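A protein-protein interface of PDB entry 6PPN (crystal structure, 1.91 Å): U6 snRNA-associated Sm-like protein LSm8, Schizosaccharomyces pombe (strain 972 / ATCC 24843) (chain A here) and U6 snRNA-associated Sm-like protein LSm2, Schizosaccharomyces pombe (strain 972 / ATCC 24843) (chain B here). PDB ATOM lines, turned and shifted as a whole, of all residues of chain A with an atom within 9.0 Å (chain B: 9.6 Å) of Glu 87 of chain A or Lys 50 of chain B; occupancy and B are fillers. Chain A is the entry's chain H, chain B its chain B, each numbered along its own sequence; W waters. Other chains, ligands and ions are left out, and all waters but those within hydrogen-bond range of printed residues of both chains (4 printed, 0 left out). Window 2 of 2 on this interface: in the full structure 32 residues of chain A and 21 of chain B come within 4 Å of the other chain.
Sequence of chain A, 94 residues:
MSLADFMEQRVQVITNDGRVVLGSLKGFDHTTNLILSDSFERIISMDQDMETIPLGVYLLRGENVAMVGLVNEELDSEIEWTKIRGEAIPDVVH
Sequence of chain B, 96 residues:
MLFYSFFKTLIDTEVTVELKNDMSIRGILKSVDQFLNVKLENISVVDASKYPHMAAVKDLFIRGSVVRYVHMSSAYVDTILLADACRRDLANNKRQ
Water W1 bridges O of Pro 90 of chain A and ND2 of Asn 21 of chain B. Water W4 lies within hydrogen-bond range of the guanidinium group of Arg 42 of chain A and the backbone carbonyl oxygen of His 53 of chain B. Water W2 lies within hydrogen-bond range of the backbone carbonyl oxygen of Arg 85 of chain A (2.9 Å) and the backbone carbonyl oxygen of Ser 49 of chain B (3.0 Å). Water W3 lies within hydrogen-bond range of the backbone carbonyl oxygen of Arg 42 of chain A, the backbone NH of Ile 44 of chain A and a ring nitrogen (NE2) of His 53 of chain B.
Hydrophobic or aromatic side chains of chain A that line the printed part of chain B: Val 20, Ile 44, Ile 89 and Pro 90. Of the 14 printed residues of chain B, 6 touch a printed residue of chain A. Among the printed residues, 11 pairs touch across the chains. Among the printed residues, Asp or Glu carboxylates within 4 Å of a Lys or Arg side-chain nitrogen of the other chain: Glu 87 of chain A with Lys 50 of chain B (3.2 Å).
The side-chain amide oxygen of Asn 21 of chain B sits close to the backbone NH of Met 23 of chain B, 3.2 Å away. OD1 of Asp 47 of chain B sits close to N of Lys 50 of chain B, 3.3 Å away. The backbone NH of Arg 42 of chain A lies within hydrogen-bond range of the backbone carbonyl oxygen of Val 20 of chain A (2.9 Å). The backbone NH (N) of Gly 86 of chain A lies within hydrogen-bond range of the backbone carbonyl oxygen (O) of Ser 45 of chain A. The backbone carbonyl oxygen of Gly 86 of chain A sits at hydrogen-bond distance from the backbone NH of Met 46 of chain A (3.0 Å). O of Asp 47 of chain A sits at hydrogen-bond distance from NH1 of Arg 85 of chain A (3.5 Å).
OE2 of Glu 87 of chain A lies within salt-bridge range of NZ of Lys 50 of chain B, at 3.2 Å.
Printed residues of chain B within 4 Å of Val 20 of chain A: His 53 (3.9 Å). Asp 47 of chain A touches none of the printed residues of chain B. Of the printed residues of chain B, Arg 85 of chain A touches Pro 52. Of chain B, only Lys 50 and His 53 come within 4 Å of Glu 87 of chain A. No residue of chain B comes within 4 Å of Ala 88 of chain A. Of the printed residues of chain A, Asn 21 of chain B touches Ile 89 and Pro 90. Of the printed residues of chain A, Met 23 of chain B touches Ile 89. No residue of chain A comes within 4 Å of Ser 49 of chain B. Lys 50 of chain B touches just one residue of chain A: Glu 87. Of chain A, only Pro 90 comes within 4 Å of Tyr 51 of chain B. Printed residues of chain A within 4 Å of Pro 52 of chain B: Arg 85 (3.4 Å) and Gly 86 (3.99 Å). The nearest residue of chain A that does not touch Lys 50 of chain B is Gly 86 of chain A (4.2 Å). The nearest printed residue of chain B that does not touch Val 20 of chain A is Met 54 of chain B (7.3 Å).
Val 20 of chain A touches His 53 of chain B (CG2 to CD2, 3.9 Å). Ile 44 of chain A touches His 53 of chain B. Arg 85 of chain A touches Pro 52 of chain B (O to CG, 3.4 Å). CA of Gly 86 of chain A touches CD of Pro 52 of chain B, at 3.99 Å. Glu 87 of chain A touches His 53 of chain B (O to CE1, 3.3 Å). ND2 of Asn 21 of chain B touches CG2 of Ile 89 of chain A, 3.8 Å away. Met 23 of chain B touches Ile 89 of chain A (SD to CG2, 3.8 Å). Ile 89 of chain A touches His 53 of chain B (CG1 to CE1, 3.8 Å). Pro 90 of chain A touches Asn 21 of chain B. Pro 90 of chain A touches Tyr 51 of chain B.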
ATOM      1  N   GLY A  18      17.115 -10.858  24.978  1.00  0.00           N
ATOM      2  CA  GLY A  18      16.917  -9.435  24.751  1.00  0.00           C
ATOM      3  C   GLY A  18      17.705  -8.854  23.598  1.00  0.00           C
ATOM      4  O   GLY A  18      17.666  -7.638  23.391  1.00  0.00           O
ATOM      5  N   VAL A  20      18.872  -7.929  19.699  1.00  0.00           N
ATOM      6  CA  VAL A  20      18.179  -7.516  18.485  1.00  0.00           C
ATOM      7  C   VAL A  20      19.126  -7.812  17.334  1.00  0.00           C
ATOM      8  O   VAL A  20      20.216  -7.237  17.279  1.00  0.00           O
ATOM      9  CB  VAL A  20      17.823  -6.020  18.527  1.00  0.00           C
ATOM     10  CG1 VAL A  20      17.158  -5.586  17.213  1.00  0.00           C
ATOM     11  CG2 VAL A  20      16.893  -5.736  19.706  1.00  0.00           C
ATOM     12  N   ARG A  42      22.048  -5.025  16.776  1.00  0.00           N
ATOM     13  CA  ARG A  42      21.889  -3.629  17.169  1.00  0.00           C
ATOM     14  C   ARG A  42      21.791  -3.569  18.681  1.00  0.00           C
ATOM     15  O   ARG A  42      20.999  -4.304  19.283  1.00  0.00           O
ATOM     16  CB  ARG A  42      20.626  -3.004  16.570  1.00  0.00           C
ATOM     17  CG  ARG A  42      20.815  -2.250  15.298  1.00  0.00           C
ATOM     18  CD  ARG A  42      19.451  -1.856  14.706  1.00  0.00           C
ATOM     19  NE  ARG A  42      19.642  -1.195  13.413  1.00  0.00           N
ATOM     20  CZ  ARG A  42      18.691  -1.021  12.504  1.00  0.00           C
ATOM     21  NH1 ARG A  42      17.466  -1.458  12.735  1.00  0.00           N
ATOM     22  NH2 ARG A  42      18.971  -0.410  11.356  1.00  0.00           N
ATOM     23  N   ILE A  43      22.612  -2.732  19.288  1.00  0.00           N
ATOM     24  CA  ILE A  43      22.547  -2.489  20.720  1.00  0.00           C
ATOM     25  C   ILE A  43      22.098  -1.048  20.899  1.00  0.00           C
ATOM     26  O   ILE A  43      22.891  -0.108  20.759  1.00  0.00           O
ATOM     27  CB  ILE A  43      23.877  -2.769  21.420  1.00  0.00           C
ATOM     28  CG1 ILE A  43      24.318  -4.212  21.130  1.00  0.00           C
ATOM     29  CG2 ILE A  43      23.728  -2.535  22.905  1.00  0.00           C
ATOM     30  CD1 ILE A  43      25.650  -4.576  21.727  1.00  0.00           C
ATOM     31  N   ILE A  44      20.806  -0.884  21.115  1.00  0.00           N
ATOM     32  CA  ILE A  44      20.191   0.367  21.539  1.00  0.00           C
ATOM     33  C   ILE A  44      20.213   0.405  23.057  1.00  0.00           C
ATOM     34  O   ILE A  44      19.917  -0.593  23.719  1.00  0.00           O
ATOM     35  CB  ILE A  44      18.750   0.469  21.002  1.00  0.00           C
ATOM     36  CG1 ILE A  44      18.762   0.703  19.501  1.00  0.00           C
ATOM     37  CG2 ILE A  44      17.907   1.501  21.780  1.00  0.00           C
ATOM     38  CD1 ILE A  44      17.412   0.471  18.878  1.00  0.00           C
ATOM     39  N   SER A  45      20.591   1.549  23.612  1.00  0.00           N
ATOM     40  CA  SER A  45      20.650   1.746  25.047  1.00  0.00           C
ATOM     41  C   SER A  45      20.125   3.142  25.361  1.00  0.00           C
ATOM     42  O   SER A  45      19.750   3.906  24.469  1.00  0.00           O
ATOM     43  CB  SER A  45      22.073   1.581  25.555  1.00  0.00           C
ATOM     44  OG  SER A  45      22.807   2.745  25.240  1.00  0.00           O
ATOM     45  N   MET A  46      20.105   3.496  26.638  1.00  0.00           N
ATOM     46  CA  MET A  46      19.803   4.878  26.971  1.00  0.00           C
ATOM     47  C   MET A  46      21.038   5.712  27.197  1.00  0.00           C
ATOM     48  O   MET A  46      21.012   6.910  26.903  1.00  0.00           O
ATOM     49  CB  MET A  46      18.882   4.970  28.187  1.00  0.00           C
ATOM     50  CG  MET A  46      17.438   4.708  27.799  1.00  0.00           C
ATOM     51  SD  MET A  46      16.398   4.579  29.227  1.00  0.00           S
ATOM     52  CE  MET A  46      17.163   3.190  30.063  1.00  0.00           C
ATOM     53  N   ASP A  47      22.131   5.108  27.666  1.00  0.00           N
ATOM     54  CA  ASP A  47      23.289   5.907  28.057  1.00  0.00           C
ATOM     55  C   ASP A  47      24.174   6.267  26.865  1.00  0.00           C
ATOM     56  O   ASP A  47      24.814   7.322  26.880  1.00  0.00           O
ATOM     57  CB  ASP A  47      24.108   5.159  29.114  1.00  0.00           C
ATOM     58  N   ILE A  84      19.358   7.025  18.290  1.00  0.00           N
ATOM     59  CA  ILE A  84      18.202   6.400  18.938  1.00  0.00           C
ATOM     60  C   ILE A  84      18.609   5.807  20.282  1.00  0.00           C
ATOM     61  O   ILE A  84      19.606   5.080  20.386  1.00  0.00           O
ATOM     62  CB  ILE A  84      17.555   5.326  18.044  1.00  0.00           C
ATOM     63  CG1 ILE A  84      16.686   5.974  16.966  1.00  0.00           C
ATOM     64  CG2 ILE A  84      16.704   4.350  18.885  1.00  0.00           C
ATOM     65  CD1 ILE A  84      15.231   6.180  17.393  1.00  0.00           C
ATOM     66  N   ARG A  85      17.815   6.099  21.305  1.00  0.00           N
ATOM     67  CA  ARG A  85      18.022   5.597  22.652  1.00  0.00           C
ATOM     68  C   ARG A  85      16.790   4.840  23.096  1.00  0.00           C
ATOM     69  O   ARG A  85      15.675   5.109  22.642  1.00  0.00           O
ATOM     70  CB  ARG A  85      18.279   6.718  23.633  1.00  0.00           C
ATOM     71  CG  ARG A  85      19.398   7.615  23.209  1.00  0.00           C
ATOM     72  CD  ARG A  85      20.673   6.835  23.053  1.00  0.00           C
ATOM     73  NE  ARG A  85      21.757   7.732  22.703  1.00  0.00           N
ATOM     74  CZ  ARG A  85      22.436   8.435  23.599  1.00  0.00           C
ATOM     75  NH1 ARG A  85      22.129   8.324  24.888  1.00  0.00           N
ATOM     76  NH2 ARG A  85      23.405   9.247  23.213  1.00  0.00           N
ATOM     77  N   GLY A  86      17.004   3.872  23.963  1.00  0.00           N
ATOM     78  CA  GLY A  86      15.895   3.053  24.409  1.00  0.00           C
ATOM     79  C   GLY A  86      16.361   2.159  25.531  1.00  0.00           C
ATOM     80  O   GLY A  86      17.549   2.092  25.855  1.00  0.00           O
ATOM     81  N   GLU A  87      15.401   1.505  26.155  1.00  0.00           N
ATOM     82  CA  GLU A  87      15.747   0.615  27.241  1.00  0.00           C
ATOM     83  C   GLU A  87      16.190  -0.716  26.670  1.00  0.00           C
ATOM     84  O   GLU A  87      15.779  -1.108  25.572  1.00  0.00           O
ATOM     85  CB  GLU A  87      14.549   0.435  28.164  1.00  0.00           C
ATOM     86  CG  GLU A  87      14.157   1.744  28.776  1.00  0.00           C
ATOM     87  CD  GLU A  87      13.164   1.604  29.876  1.00  0.00           C
ATOM     88  OE1 GLU A  87      12.643   2.645  30.324  1.00  0.00           O
ATOM     89  OE2 GLU A  87      12.905   0.459  30.294  1.00  0.00           O
ATOM     90  N   ALA A  88      17.048  -1.410  27.413  1.00  0.00           N
ATOM     91  CA  ALA A  88      17.379  -2.776  27.041  1.00  0.00           C
ATOM     92  C   ALA A  88      16.116  -3.611  27.069  1.00  0.00           C
ATOM     93  O   ALA A  88      15.332  -3.540  28.019  1.00  0.00           O
ATOM     94  CB  ALA A  88      18.393  -3.364  28.014  1.00  0.00           C
ATOM     95  N   ILE A  89      15.930  -4.431  26.050  1.00  0.00           N
ATOM     96  CA  ILE A  89      14.778  -5.339  26.073  1.00  0.00           C
ATOM     97  C   ILE A  89      14.988  -6.386  27.165  1.00  0.00           C
ATOM     98  O   ILE A  89      16.099  -6.943  27.283  1.00  0.00           O
ATOM     99  CB  ILE A  89      14.589  -5.982  24.699  1.00  0.00           C
ATOM    100  CG1 ILE A  89      14.319  -4.886  23.665  1.00  0.00           C
ATOM    101  CG2 ILE A  89      13.474  -7.013  24.730  1.00  0.00           C
ATOM    102  CD1 ILE A  89      13.911  -5.409  22.309  1.00  0.00           C
ATOM    103  N   PRO A  90      14.003  -6.657  28.008  1.00  0.00           N
ATOM    104  CA  PRO A  90      14.218  -7.614  29.104  1.00  0.00           C
ATOM    105  C   PRO A  90      14.373  -9.044  28.616  1.00  0.00           C
ATOM    106  O   PRO A  90      13.999  -9.404  27.499  1.00  0.00           O
ATOM    107  CB  PRO A  90      12.955  -7.465  29.945  1.00  0.00           C
ATOM    108  CG  PRO A  90      12.474  -6.047  29.649  1.00  0.00           C
ATOM    109  CD  PRO A  90      12.752  -5.886  28.186  1.00  0.00           C
ATOM    110  N   ASN B  21       8.733 -11.526  28.211  1.00  0.00           N
ATOM    111  CA  ASN B  21       9.724 -10.495  28.523  1.00  0.00           C
ATOM    112  C   ASN B  21       9.070  -9.179  28.871  1.00  0.00           C
ATOM    113  O   ASN B  21       9.729  -8.142  28.834  1.00  0.00           O
ATOM    114  CB  ASN B  21      10.725 -10.297  27.372  1.00  0.00           C
ATOM    115  CG  ASN B  21      10.066  -9.870  26.084  1.00  0.00           C
ATOM    116  OD1 ASN B  21       8.872  -9.594  26.049  1.00  0.00           O
ATOM    117  ND2 ASN B  21      10.847  -9.814  25.005  1.00  0.00           N
ATOM    118  N   ASP B  22       7.770  -9.198  29.151  1.00  0.00           N
ATOM    119  CA  ASP B  22       6.954  -8.075  29.622  1.00  0.00           C
ATOM    120  C   ASP B  22       6.621  -7.074  28.506  1.00  0.00           C
ATOM    121  O   ASP B  22       5.823  -6.156  28.762  1.00  0.00           O
ATOM    122  CB  ASP B  22       7.594  -7.347  30.820  1.00  0.00           C
ATOM    123  CG  ASP B  22       7.579  -8.204  32.086  1.00  0.00           C
ATOM    124  OD1 ASP B  22       7.077  -9.358  32.027  1.00  0.00           O
ATOM    125  OD2 ASP B  22       8.070  -7.743  33.136  1.00  0.00           O
ATOM    126  N   MET B  23       7.127  -7.253  27.279  1.00  0.00           N
ATOM    127  CA  MET B  23       6.616  -6.497  26.141  1.00  0.00           C
ATOM    128  C   MET B  23       5.215  -6.953  25.774  1.00  0.00           C
ATOM    129  O   MET B  23       4.876  -8.139  25.844  1.00  0.00           O
ATOM    130  CB  MET B  23       7.516  -6.654  24.907  1.00  0.00           C
ATOM    131  CG  MET B  23       8.920  -6.131  25.130  1.00  0.00           C
ATOM    132  SD  MET B  23       9.928  -6.232  23.613  1.00  0.00           S
ATOM    133  CE  MET B  23       8.918  -5.275  22.481  1.00  0.00           C
ATOM    134  N   SER B  24       4.419  -5.995  25.310  1.00  0.00           N
ATOM    135  CA  SER B  24       3.091  -6.243  24.797  1.00  0.00           C
ATOM    136  C   SER B  24       2.979  -5.647  23.404  1.00  0.00           C
ATOM    137  O   SER B  24       3.387  -4.502  23.178  1.00  0.00           O
ATOM    138  CB  SER B  24       2.041  -5.623  25.721  1.00  0.00           C
ATOM    139  OG  SER B  24       1.961  -6.359  26.927  1.00  0.00           O
ATOM    140  N   VAL B  45       3.908  -1.572  19.253  1.00  0.00           N
ATOM    141  CA  VAL B  45       4.331  -1.931  20.602  1.00  0.00           C
ATOM    142  C   VAL B  45       3.627  -1.020  21.599  1.00  0.00           C
ATOM    143  O   VAL B  45       3.568   0.202  21.419  1.00  0.00           O
ATOM    144  CB  VAL B  45       5.855  -1.819  20.725  1.00  0.00           C
ATOM    145  CG1 VAL B  45       6.290  -2.137  22.126  1.00  0.00           C
ATOM    146  CG2 VAL B  45       6.521  -2.754  19.736  1.00  0.00           C
ATOM    147  N   VAL B  46       3.092  -1.612  22.664  1.00  0.00           N
ATOM    148  CA  VAL B  46       2.249  -0.840  23.575  1.00  0.00           C
ATOM    149  C   VAL B  46       3.000   0.347  24.152  1.00  0.00           C
ATOM    150  O   VAL B  46       2.507   1.482  24.126  1.00  0.00           O
ATOM    151  CB  VAL B  46       1.687  -1.743  24.683  1.00  0.00           C
ATOM    152  CG1 VAL B  46       1.118  -0.884  25.820  1.00  0.00           C
ATOM    153  CG2 VAL B  46       0.644  -2.675  24.085  1.00  0.00           C
ATOM    154  N   ASP B  47       4.212   0.135  24.639  1.00  0.00           N
ATOM    155  CA  ASP B  47       4.956   1.242  25.263  1.00  0.00           C
ATOM    156  C   ASP B  47       6.117   1.637  24.352  1.00  0.00           C
ATOM    157  O   ASP B  47       7.292   1.410  24.656  1.00  0.00           O
ATOM    158  CB  ASP B  47       5.433   0.816  26.638  1.00  0.00           C
ATOM    159  CG  ASP B  47       5.925   1.945  27.458  1.00  0.00           C
ATOM    160  OD1 ASP B  47       6.532   2.882  26.908  1.00  0.00           O
ATOM    161  OD2 ASP B  47       5.713   1.879  28.680  1.00  0.00           O
ATOM    162  N   ALA B  48       5.780   2.284  23.237  1.00  0.00           N
ATOM    163  CA  ALA B  48       6.740   2.348  22.140  1.00  0.00           C
ATOM    164  C   ALA B  48       7.942   3.213  22.473  1.00  0.00           C
ATOM    165  O   ALA B  48       9.023   2.996  21.920  1.00  0.00           O
ATOM    166  CB  ALA B  48       6.057   2.845  20.872  1.00  0.00           C
ATOM    167  N   SER B  49       7.797   4.193  23.358  1.00  0.00           N
ATOM    168  CA  SER B  49       8.970   4.979  23.701  1.00  0.00           C
ATOM    169  C   SER B  49       9.911   4.199  24.605  1.00  0.00           C
ATOM    170  O   SER B  49      11.118   4.448  24.597  1.00  0.00           O
ATOM    171  CB  SER B  49       8.558   6.285  24.363  1.00  0.00           C
ATOM    172  OG  SER B  49       8.234   6.036  25.709  1.00  0.00           O
ATOM    173  N   LYS B  50       9.387   3.237  25.367  1.00  0.00           N
ATOM    174  CA  LYS B  50      10.265   2.299  26.060  1.00  0.00           C
ATOM    175  C   LYS B  50      11.045   1.446  25.066  1.00  0.00           C
ATOM    176  O   LYS B  50      12.247   1.222  25.241  1.00  0.00           O
ATOM    177  CB  LYS B  50       9.438   1.418  26.998  1.00  0.00           C
ATOM    178  CG  LYS B  50      10.113   1.000  28.297  1.00  0.00           C
ATOM    179  CD  LYS B  50       9.308  -0.135  28.960  1.00  0.00           C
ATOM    180  CE  LYS B  50       8.803   0.246  30.342  1.00  0.00           C
ATOM    181  NZ  LYS B  50       9.876   0.172  31.377  1.00  0.00           N
ATOM    182  N   TYR B  51      10.378   0.962  24.011  1.00  0.00           N
ATOM    183  CA  TYR B  51      10.953   0.021  23.051  1.00  0.00           C
ATOM    184  C   TYR B  51      10.835   0.596  21.646  1.00  0.00           C
ATOM    185  O   TYR B  51       9.939   0.206  20.880  1.00  0.00           O
ATOM    186  CB  TYR B  51      10.267  -1.335  23.129  1.00  0.00           C
ATOM    187  CG  TYR B  51      10.248  -1.906  24.524  1.00  0.00           C
ATOM    188  CD1 TYR B  51      11.434  -2.159  25.191  1.00  0.00           C
ATOM    189  CD2 TYR B  51       9.044  -2.219  25.169  1.00  0.00           C
ATOM    190  CE1 TYR B  51      11.433  -2.690  26.469  1.00  0.00           C
ATOM    191  CE2 TYR B  51       9.036  -2.752  26.456  1.00  0.00           C
ATOM    192  CZ  TYR B  51      10.239  -2.984  27.090  1.00  0.00           C
ATOM    193  OH  TYR B  51      10.280  -3.514  28.353  1.00  0.00           O
ATOM    194  N   PRO B  52      11.732   1.504  21.259  1.00  0.00           N
ATOM    195  CA  PRO B  52      11.682   2.045  19.897  1.00  0.00           C
ATOM    196  C   PRO B  52      12.225   1.091  18.850  1.00  0.00           C
ATOM    197  O   PRO B  52      12.197   1.428  17.663  1.00  0.00           O
ATOM    198  CB  PRO B  52      12.556   3.292  19.996  1.00  0.00           C
ATOM    199  CG  PRO B  52      13.579   2.916  21.022  1.00  0.00           C
ATOM    200  CD  PRO B  52      12.897   1.988  22.008  1.00  0.00           C
ATOM    201  N   HIS B  53      12.630  -0.116  19.253  1.00  0.00           N
ATOM    202  CA  HIS B  53      13.328  -1.027  18.361  1.00  0.00           C
ATOM    203  C   HIS B  53      12.466  -1.481  17.200  1.00  0.00           C
ATOM    204  O   HIS B  53      13.008  -1.844  16.148  1.00  0.00           O
ATOM    205  CB  HIS B  53      13.806  -2.272  19.101  1.00  0.00           C
ATOM    206  CG  HIS B  53      14.469  -1.992  20.404  1.00  0.00           C
ATOM    207  ND1 HIS B  53      13.794  -1.454  21.483  1.00  0.00           N
ATOM    208  CD2 HIS B  53      15.745  -2.182  20.813  1.00  0.00           C
ATOM    209  CE1 HIS B  53      14.630  -1.330  22.501  1.00  0.00           C
ATOM    210  NE2 HIS B  53      15.821  -1.756  22.118  1.00  0.00           N
ATOM    211  N   MET B  54      11.143  -1.461  17.346  1.00  0.00           N
ATOM    212  CA  MET B  54      10.274  -2.036  16.335  1.00  0.00           C
ATOM    213  C   MET B  54       9.531  -0.976  15.547  1.00  0.00           C
ATOM    214  O   MET B  54       8.482  -1.261  14.950  1.00  0.00           O
ATOM    215  CB  MET B  54       9.317  -3.005  17.017  1.00  0.00           C
ATOM    216  CG  MET B  54      10.086  -3.833  18.025  1.00  0.00           C
ATOM    217  SD  MET B  54       9.472  -5.479  18.204  1.00  0.00           S
ATOM    218  CE  MET B  54       9.257  -6.013  16.509  1.00  0.00           C
HETATM  219  O   HOH W   1      13.385 -10.684  25.221  1.00  0.00           O
HETATM  220  O   HOH W   2      12.833   5.798  22.580  1.00  0.00           O
HETATM  221  O   HOH W   3      18.672  -3.106  20.652  1.00  0.00           O
HETATM  222  O   HOH W   4      16.168  -1.888  15.247  1.00  0.00           O
